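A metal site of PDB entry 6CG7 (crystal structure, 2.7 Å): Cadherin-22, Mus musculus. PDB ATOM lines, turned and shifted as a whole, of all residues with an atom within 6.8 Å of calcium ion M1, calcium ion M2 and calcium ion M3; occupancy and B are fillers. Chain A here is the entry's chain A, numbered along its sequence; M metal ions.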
ATOM      1  N   GLU A  11       1.873  13.050  19.858  1.00  0.00           N
ATOM      2  CA  GLU A  11       3.083  13.837  19.907  1.00  0.00           C
ATOM      3  C   GLU A  11       3.582  13.973  21.353  1.00  0.00           C
ATOM      4  O   GLU A  11       2.888  13.631  22.314  1.00  0.00           O
ATOM      5  CB  GLU A  11       2.869  15.238  19.317  1.00  0.00           C
ATOM      6  CG  GLU A  11       1.915  16.120  20.115  1.00  0.00           C
ATOM      7  CD  GLU A  11       2.014  17.587  19.711  1.00  0.00           C
ATOM      8  OE1 GLU A  11       0.971  18.279  19.704  1.00  0.00           O
ATOM      9  OE2 GLU A  11       3.138  18.046  19.414  1.00  0.00           O
ATOM     10  N   GLU A  12       4.803  14.479  21.472  1.00  0.00           N
ATOM     11  CA  GLU A  12       5.417  14.794  22.755  1.00  0.00           C
ATOM     12  C   GLU A  12       5.306  13.627  23.738  1.00  0.00           C
ATOM     13  O   GLU A  12       4.965  13.797  24.904  1.00  0.00           O
ATOM     14  CB  GLU A  12       4.805  16.063  23.358  1.00  0.00           C
ATOM     15  CG  GLU A  12       4.606  17.210  22.387  1.00  0.00           C
ATOM     16  CD  GLU A  12       5.916  17.770  21.861  1.00  0.00           C
ATOM     17  OE1 GLU A  12       6.961  17.523  22.495  1.00  0.00           O
ATOM     18  OE2 GLU A  12       5.904  18.447  20.805  1.00  0.00           O
ATOM     19  N   LEU A  63       7.958  12.962  19.150  1.00  0.00           N
ATOM     20  CA  LEU A  63       7.467  13.622  17.946  1.00  0.00           C
ATOM     21  C   LEU A  63       6.814  14.958  18.312  1.00  0.00           C
ATOM     22  O   LEU A  63       6.266  15.120  19.404  1.00  0.00           O
ATOM     23  CB  LEU A  63       6.469  12.736  17.212  1.00  0.00           C
ATOM     24  CG  LEU A  63       6.995  11.394  16.693  1.00  0.00           C
ATOM     25  CD1 LEU A  63       5.848  10.559  16.133  1.00  0.00           C
ATOM     26  CD2 LEU A  63       8.071  11.584  15.645  1.00  0.00           C
ATOM     27  N   ASP A  64       6.876  15.899  17.374  1.00  0.00           N
ATOM     28  CA  ASP A  64       6.346  17.246  17.564  1.00  0.00           C
ATOM     29  C   ASP A  64       5.462  17.599  16.376  1.00  0.00           C
ATOM     30  O   ASP A  64       5.957  17.762  15.265  1.00  0.00           O
ATOM     31  CB  ASP A  64       7.476  18.255  17.729  1.00  0.00           C
ATOM     32  CG  ASP A  64       6.982  19.668  17.982  1.00  0.00           C
ATOM     33  OD1 ASP A  64       5.816  19.824  18.404  1.00  0.00           O
ATOM     34  OD2 ASP A  64       7.759  20.618  17.771  1.00  0.00           O
ATOM     35  N   ARG A  65       4.147  17.723  16.621  1.00  0.00           N
ATOM     36  CA  ARG A  65       3.230  18.040  15.538  1.00  0.00           C
ATOM     37  C   ARG A  65       3.448  19.449  15.016  1.00  0.00           C
ATOM     38  O   ARG A  65       3.309  19.710  13.815  1.00  0.00           O
ATOM     39  CB  ARG A  65       1.787  17.877  16.010  1.00  0.00           C
ATOM     40  CG  ARG A  65       0.766  17.815  14.890  1.00  0.00           C
ATOM     41  CD  ARG A  65      -0.639  18.111  15.388  1.00  0.00           C
ATOM     42  NE  ARG A  65      -0.760  19.497  15.827  1.00  0.00           N
ATOM     43  CZ  ARG A  65      -0.925  20.526  15.004  1.00  0.00           C
ATOM     44  NH1 ARG A  65      -0.996  20.328  13.685  1.00  0.00           N
ATOM     45  NH2 ARG A  65      -1.026  21.758  15.486  1.00  0.00           N
ATOM     46  N   GLU A  66       3.805  20.379  15.909  1.00  0.00           N
ATOM     47  CA  GLU A  66       4.107  21.742  15.494  1.00  0.00           C
ATOM     48  C   GLU A  66       5.379  21.832  14.672  1.00  0.00           C
ATOM     49  O   GLU A  66       5.643  22.875  14.078  1.00  0.00           O
ATOM     50  CB  GLU A  66       4.192  22.666  16.715  1.00  0.00           C
ATOM     51  CG  GLU A  66       2.850  22.986  17.361  1.00  0.00           C
ATOM     52  CD  GLU A  66       2.203  21.784  18.027  1.00  0.00           C
ATOM     53  OE1 GLU A  66       2.930  20.994  18.672  1.00  0.00           O
ATOM     54  OE2 GLU A  66       0.973  21.628  17.910  1.00  0.00           O
ATOM     55  N   GLN A  67       6.189  20.771  14.647  1.00  0.00           N
ATOM     56  CA  GLN A  67       7.340  20.681  13.758  1.00  0.00           C
ATOM     57  C   GLN A  67       6.986  19.965  12.467  1.00  0.00           C
ATOM     58  O   GLN A  67       7.298  20.450  11.378  1.00  0.00           O
ATOM     59  CB  GLN A  67       8.495  19.958  14.467  1.00  0.00           C
ATOM     60  CG  GLN A  67       9.781  19.865  13.649  1.00  0.00           C
ATOM     61  CD  GLN A  67      10.541  18.569  13.890  1.00  0.00           C
ATOM     62  OE1 GLN A  67      10.050  17.655  14.557  1.00  0.00           O
ATOM     63  NE2 GLN A  67      11.747  18.485  13.335  1.00  0.00           N
ATOM     64  N   GLN A  97      -0.670  12.920  16.207  1.00  0.00           N
ATOM     65  CA  GLN A  97      -1.839  13.601  16.723  1.00  0.00           C
ATOM     66  C   GLN A  97      -1.444  14.730  17.671  1.00  0.00           C
ATOM     67  O   GLN A  97      -0.350  14.747  18.250  1.00  0.00           O
ATOM     68  CB  GLN A  97      -2.772  12.613  17.431  1.00  0.00           C
ATOM     69  CG  GLN A  97      -4.132  13.198  17.846  1.00  0.00           C
ATOM     70  CD  GLN A  97      -4.904  13.792  16.675  1.00  0.00           C
ATOM     71  OE1 GLN A  97      -5.160  14.992  16.629  1.00  0.00           O
ATOM     72  NE2 GLN A  97      -5.283  12.943  15.733  1.00  0.00           N
ATOM     73  N   ASP A  98      -2.356  15.689  17.835  1.00  0.00           N
ATOM     74  CA  ASP A  98      -2.104  16.917  18.555  1.00  0.00           C
ATOM     75  C   ASP A  98      -2.381  16.763  20.048  1.00  0.00           C
ATOM     76  O   ASP A  98      -3.283  16.021  20.448  1.00  0.00           O
ATOM     77  CB  ASP A  98      -2.983  18.045  17.994  1.00  0.00           C
ATOM     78  CG  ASP A  98      -2.830  19.340  18.739  1.00  0.00           C
ATOM     79  OD1 ASP A  98      -1.729  19.933  18.663  1.00  0.00           O
ATOM     80  OD2 ASP A  98      -3.793  19.768  19.399  1.00  0.00           O
ATOM     81  N   ILE A  99      -1.582  17.459  20.852  1.00  0.00           N
ATOM     82  CA  ILE A  99      -1.873  17.657  22.268  1.00  0.00           C
ATOM     83  C   ILE A  99      -1.767  19.150  22.546  1.00  0.00           C
ATOM     84  O   ILE A  99      -1.091  19.903  21.843  1.00  0.00           O
ATOM     85  CB  ILE A  99      -0.918  16.874  23.201  1.00  0.00           C
ATOM     86  CG1 ILE A  99       0.498  17.457  23.166  1.00  0.00           C
ATOM     87  CG2 ILE A  99      -0.918  15.389  22.829  1.00  0.00           C
ATOM     88  CD1 ILE A  99       1.451  16.851  24.155  1.00  0.00           C
ATOM     89  N   ASN A 100      -2.463  19.589  23.596  1.00  0.00           N
ATOM     90  CA  ASN A 100      -2.481  21.004  23.978  1.00  0.00           C
ATOM     91  C   ASN A 100      -1.174  21.332  24.693  1.00  0.00           C
ATOM     92  O   ASN A 100      -1.082  21.356  25.930  1.00  0.00           O
ATOM     93  CB  ASN A 100      -3.685  21.314  24.841  1.00  0.00           C
ATOM     94  CG  ASN A 100      -3.804  22.786  25.162  1.00  0.00           C
ATOM     95  OD1 ASN A 100      -3.296  23.634  24.430  1.00  0.00           O
ATOM     96  ND2 ASN A 100      -4.468  23.106  26.273  1.00  0.00           N
ATOM     97  N   ASP A 101      -0.138  21.611  23.894  1.00  0.00           N
ATOM     98  CA  ASP A 101       1.175  21.969  24.430  1.00  0.00           C
ATOM     99  C   ASP A 101       1.689  23.281  23.842  1.00  0.00           C
ATOM    100  O   ASP A 101       2.901  23.528  23.866  1.00  0.00           O
ATOM    101  CB  ASP A 101       2.182  20.847  24.186  1.00  0.00           C
ATOM    102  CG  ASP A 101       2.474  20.645  22.705  1.00  0.00           C
ATOM    103  OD1 ASP A 101       3.643  20.375  22.366  1.00  0.00           O
ATOM    104  OD2 ASP A 101       1.535  20.748  21.893  1.00  0.00           O
ATOM    105  N   SER A 102       0.809  24.131  23.323  1.00  0.00           N
ATOM    106  CA  SER A 102       1.180  25.434  22.784  1.00  0.00           C
ATOM    107  C   SER A 102       0.362  26.508  23.478  1.00  0.00           C
ATOM    108  O   SER A 102      -0.867  26.488  23.417  1.00  0.00           O
ATOM    109  CB  SER A 102       0.956  25.477  21.266  1.00  0.00           C
ATOM    110  OG  SER A 102       1.631  24.423  20.613  1.00  0.00           O
ATOM    111  N   GLU A 103       1.042  27.447  24.138  1.00  0.00           N
ATOM    112  CA  GLU A 103       0.357  28.536  24.811  1.00  0.00           C
ATOM    113  C   GLU A 103      -0.213  29.525  23.785  1.00  0.00           C
ATOM    114  O   GLU A 103       0.364  29.707  22.710  1.00  0.00           O
ATOM    115  CB  GLU A 103       1.296  29.276  25.754  1.00  0.00           C
ATOM    116  CG  GLU A 103       1.708  28.511  26.997  1.00  0.00           C
ATOM    117  CD  GLU A 103       2.254  29.416  28.085  1.00  0.00           C
ATOM    118  OE1 GLU A 103       2.244  30.657  27.900  1.00  0.00           O
ATOM    119  OE2 GLU A 103       2.693  28.893  29.129  1.00  0.00           O
ATOM    120  N   PRO A 104      -1.340  30.169  24.096  1.00  0.00           N
ATOM    121  CA  PRO A 104      -1.790  31.273  23.250  1.00  0.00           C
ATOM    122  C   PRO A 104      -0.818  32.432  23.312  1.00  0.00           C
ATOM    123  O   PRO A 104      -0.250  32.733  24.363  1.00  0.00           O
ATOM    124  CB  PRO A 104      -3.161  31.652  23.840  1.00  0.00           C
ATOM    125  CG  PRO A 104      -3.569  30.472  24.642  1.00  0.00           C
ATOM    126  CD  PRO A 104      -2.308  29.871  25.165  1.00  0.00           C
ATOM    127  N   ASP A 132      -2.944  30.260  18.524  1.00  0.00           N
ATOM    128  CA  ASP A 132      -2.597  29.016  19.213  1.00  0.00           C
ATOM    129  C   ASP A 132      -2.084  28.036  18.179  1.00  0.00           C
ATOM    130  O   ASP A 132      -2.798  27.696  17.226  1.00  0.00           O
ATOM    131  CB  ASP A 132      -3.810  28.445  19.951  1.00  0.00           C
ATOM    132  CG  ASP A 132      -3.433  27.417  20.992  1.00  0.00           C
ATOM    133  OD1 ASP A 132      -3.809  27.598  22.164  1.00  0.00           O
ATOM    134  OD2 ASP A 132      -2.761  26.423  20.641  1.00  0.00           O
ATOM    135  N   ALA A 133      -0.843  27.580  18.356  1.00  0.00           N
ATOM    136  CA  ALA A 133      -0.205  26.722  17.361  1.00  0.00           C
ATOM    137  C   ALA A 133      -0.753  25.302  17.362  1.00  0.00           C
ATOM    138  O   ALA A 133      -0.340  24.508  16.510  1.00  0.00           O
ATOM    139  CB  ALA A 133       1.306  26.683  17.604  1.00  0.00           C
ATOM    140  N   ASP A 134      -1.655  24.959  18.280  1.00  0.00           N
ATOM    141  CA  ASP A 134      -2.198  23.615  18.341  1.00  0.00           C
ATOM    142  C   ASP A 134      -3.214  23.408  17.214  1.00  0.00           C
ATOM    143  O   ASP A 134      -3.477  24.294  16.400  1.00  0.00           O
ATOM    144  CB  ASP A 134      -2.817  23.359  19.712  1.00  0.00           C
ATOM    145  CG  ASP A 134      -1.776  23.328  20.828  1.00  0.00           C
ATOM    146  OD1 ASP A 134      -0.639  22.880  20.561  1.00  0.00           O
ATOM    147  OD2 ASP A 134      -2.093  23.746  21.955  1.00  0.00           O
ATOM    148  N   ASP A 135      -3.811  22.215  17.177  1.00  0.00           N
ATOM    149  CA  ASP A 135      -4.742  21.839  16.120  1.00  0.00           C
ATOM    150  C   ASP A 135      -6.120  22.427  16.375  1.00  0.00           C
ATOM    151  O   ASP A 135      -6.785  22.039  17.357  1.00  0.00           O
ATOM    152  CB  ASP A 135      -4.837  20.312  16.006  1.00  0.00           C
ATOM    153  CG  ASP A 135      -5.526  19.865  14.727  1.00  0.00           C
ATOM    154  OD1 ASP A 135      -5.259  18.739  14.259  1.00  0.00           O
ATOM    155  OD2 ASP A 135      -6.324  20.654  14.166  1.00  0.00           O
ATOM    156  N   SER A 140     -10.492  21.227  21.797  1.00  0.00           N
ATOM    157  CA  SER A 140     -10.444  22.642  22.138  1.00  0.00           C
ATOM    158  C   SER A 140      -9.026  23.131  22.398  1.00  0.00           C
ATOM    159  O   SER A 140      -8.840  24.159  23.054  1.00  0.00           O
ATOM    160  CB  SER A 140     -11.334  22.916  23.363  1.00  0.00           C
ATOM    161  OG  SER A 140     -12.680  22.562  23.109  1.00  0.00           O
ATOM    162  N   SER A 141      -8.024  22.409  21.886  1.00  0.00           N
ATOM    163  CA  SER A 141      -6.633  22.781  22.130  1.00  0.00           C
ATOM    164  C   SER A 141      -6.297  24.163  21.581  1.00  0.00           C
ATOM    165  O   SER A 141      -5.326  24.776  22.031  1.00  0.00           O
ATOM    166  CB  SER A 141      -5.693  21.734  21.507  1.00  0.00           C
ATOM    167  OG  SER A 141      -5.935  20.450  22.035  1.00  0.00           O
ATOM    168  N   ALA A 142      -7.079  24.662  20.614  1.00  0.00           N
ATOM    169  CA  ALA A 142      -6.839  25.963  20.027  1.00  0.00           C
ATOM    170  C   ALA A 142      -8.059  26.874  20.079  1.00  0.00           C
ATOM    171  O   ALA A 142      -8.075  27.908  19.407  1.00  0.00           O
ATOM    172  CB  ALA A 142      -6.361  25.820  18.579  1.00  0.00           C
ATOM    173  N   ARG A 143      -9.094  26.502  20.835  1.00  0.00           N
ATOM    174  CA  ARG A 143     -10.274  27.339  21.006  1.00  0.00           C
ATOM    175  C   ARG A 143     -10.068  28.222  22.226  1.00  0.00           C
ATOM    176  O   ARG A 143     -10.011  27.727  23.354  1.00  0.00           O
ATOM    177  CB  ARG A 143     -11.537  26.478  21.129  1.00  0.00           C
ATOM    178  CG  ARG A 143     -11.882  25.763  19.841  1.00  0.00           C
ATOM    179  CD  ARG A 143     -13.133  24.912  19.956  1.00  0.00           C
ATOM    180  NE  ARG A 143     -13.317  24.094  18.750  1.00  0.00           N
ATOM    181  CZ  ARG A 143     -14.268  23.180  18.596  1.00  0.00           C
ATOM    182  NH1 ARG A 143     -15.146  22.953  19.571  1.00  0.00           N
ATOM    183  NH2 ARG A 143     -14.350  22.492  17.463  1.00  0.00           N
ATOM    184  N   LEU A 144      -9.946  29.527  22.009  1.00  0.00           N
ATOM    185  CA  LEU A 144      -9.481  30.455  23.019  1.00  0.00           C
ATOM    186  C   LEU A 144     -10.647  31.216  23.659  1.00  0.00           C
ATOM    187  O   LEU A 144     -11.726  31.346  23.095  1.00  0.00           O
ATOM    188  CB  LEU A 144      -8.495  31.455  22.403  1.00  0.00           C
ATOM    189  CG  LEU A 144      -7.313  30.821  21.652  1.00  0.00           C
ATOM    190  CD1 LEU A 144      -6.448  31.901  21.028  1.00  0.00           C
ATOM    191  CD2 LEU A 144      -6.489  29.930  22.563  1.00  0.00           C
ATOM    192  N   ASP A 187      -6.821  28.781  26.250  1.00  0.00           N
ATOM    193  CA  ASP A 187      -7.357  27.733  25.385  1.00  0.00           C
ATOM    194  C   ASP A 187      -8.192  26.751  26.204  1.00  0.00           C
ATOM    195  O   ASP A 187      -8.568  27.029  27.353  1.00  0.00           O
ATOM    196  CB  ASP A 187      -6.209  27.055  24.621  1.00  0.00           C
ATOM    197  CG  ASP A 187      -5.179  26.434  25.543  1.00  0.00           C
ATOM    198  OD1 ASP A 187      -5.531  26.075  26.686  1.00  0.00           O
ATOM    199  OD2 ASP A 187      -4.010  26.296  25.107  1.00  0.00           O
ATOM    200  N   MET A 188      -8.488  25.587  25.627  1.00  0.00           N
ATOM    201  CA  MET A 188      -9.398  24.615  26.231  1.00  0.00           C
ATOM    202  C   MET A 188     -10.759  25.209  26.556  1.00  0.00           C
ATOM    203  O   MET A 188     -11.472  24.702  27.428  1.00  0.00           O
ATOM    204  CB  MET A 188      -8.782  23.990  27.494  1.00  0.00           C
ATOM    205  CG  MET A 188      -7.519  23.190  27.258  1.00  0.00           C
ATOM    206  SD  MET A 188      -7.729  21.756  26.187  1.00  0.00           S
ATOM    207  CE  MET A 188      -8.932  20.798  27.116  1.00  0.00           C
ATOM    208  N   LEU A 195      -3.977  26.393  28.844  1.00  0.00           N
ATOM    209  CA  LEU A 195      -2.823  27.268  28.787  1.00  0.00           C
ATOM    210  C   LEU A 195      -3.257  28.714  28.521  1.00  0.00           C
ATOM    211  O   LEU A 195      -4.354  28.969  28.008  1.00  0.00           O
ATOM    212  CB  LEU A 195      -1.857  26.792  27.703  1.00  0.00           C
ATOM    213  CG  LEU A 195      -1.479  25.310  27.772  1.00  0.00           C
ATOM    214  CD1 LEU A 195      -0.614  24.913  26.589  1.00  0.00           C
ATOM    215  CD2 LEU A 195      -0.778  24.994  29.081  1.00  0.00           C
HETATM  216 CA    CA M   1      -3.152  25.541  23.014  1.00  0.00          CA
HETATM  217 CA    CA M   2       0.162  20.705  19.944  1.00  0.00          CA
HETATM  218 CA    CA M   3       4.416  20.190  20.163  1.00  0.00          CA
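Calcium ion M2 is bound by the side-chain carboxylate of Glu 66 (2.4 Å), the side-chain carboxylate of Asp 101 (2.4 Å), the side-chain carboxylate of Asp 134 (2.4 Å), the side-chain carboxylate of Asp 98 (2.4 Å), the backbone carbonyl oxygen of Ile 99 (2.4 Å) and the side-chain carboxylate of Glu 11 (2.6 Å). Slightly farther from calcium ion M2 lies the side-chain carboxylate (OE1) of Glu 66 (3.1 Å).
The side-chain carboxylate (OD2) of Asp 64 lies close to the backbone NH (N) of Gln 67 (3.5 Å). The backbone NH (N) of Glu 12 sits at hydrogen-bond distance from the backbone carbonyl oxygen (O) of Leu 63 (2.6 Å). ND2 of Asn 100 sits close to SD of Met 188 (3.5 Å). The side-chain hydroxyl of Ser 141 lies close to the side-chain carboxylate of Asp 98. OD1 of Asp 98 lies close to NE of Arg 65, 3.0 Å away. N of Asp 135 lies within hydrogen-bond range of OD2 of Asp 98, at 3.3 Å. The side-chain carboxylate (OE2) of Glu 11 lies close to the backbone NH (N) of Arg 65 (3.0 Å). N of Glu 11 lies within hydrogen-bond range of O of Gln 97 (3.2 Å).
Six residues have an atom within 4 Å of calcium ion M2: Glu 11, Glu 66, Asp 98, Ile 99, Asp 101 and Asp 134. The nearest printed residue that does not touch calcium ion M2 is Ser 102 (4.1 Å).
The nearest printed residue that does not touch calcium ion M3 is Arg 65 (4.3 Å).
Calcium ion M1 is bound by OD1 of Asp 132 (2.3 Å), OD2 of Asp 134 (2.3 Å), OD1 of Asn 100 (2.4 Å), OD2 of Asp 187 (2.4 Å), O of Ser 102 (2.5 Å), O of Ser 141 (2.5 Å) and OD2 of Asp 132 (2.6 Å).
Calcium ion M3 is bound by OE1 of Glu 66 (2.3 Å), OD1 of Asp 64 (2.3 Å), OD1 of Asp 101 (2.3 Å), OE2 of Glu 12 (2.4 Å) and OE2 of Glu 11 (2.6 Å). Calcium ion M3 has five donor atoms within binding distance.
Six residues have an atom within 4 Å of calcium ion M1: Asn 100, Ser 102, Asp 132, Asp 134, Ser 141 and Asp 187. The nearest printed residue that does not touch calcium ion M1 is Leu 195 (4.4 Å).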
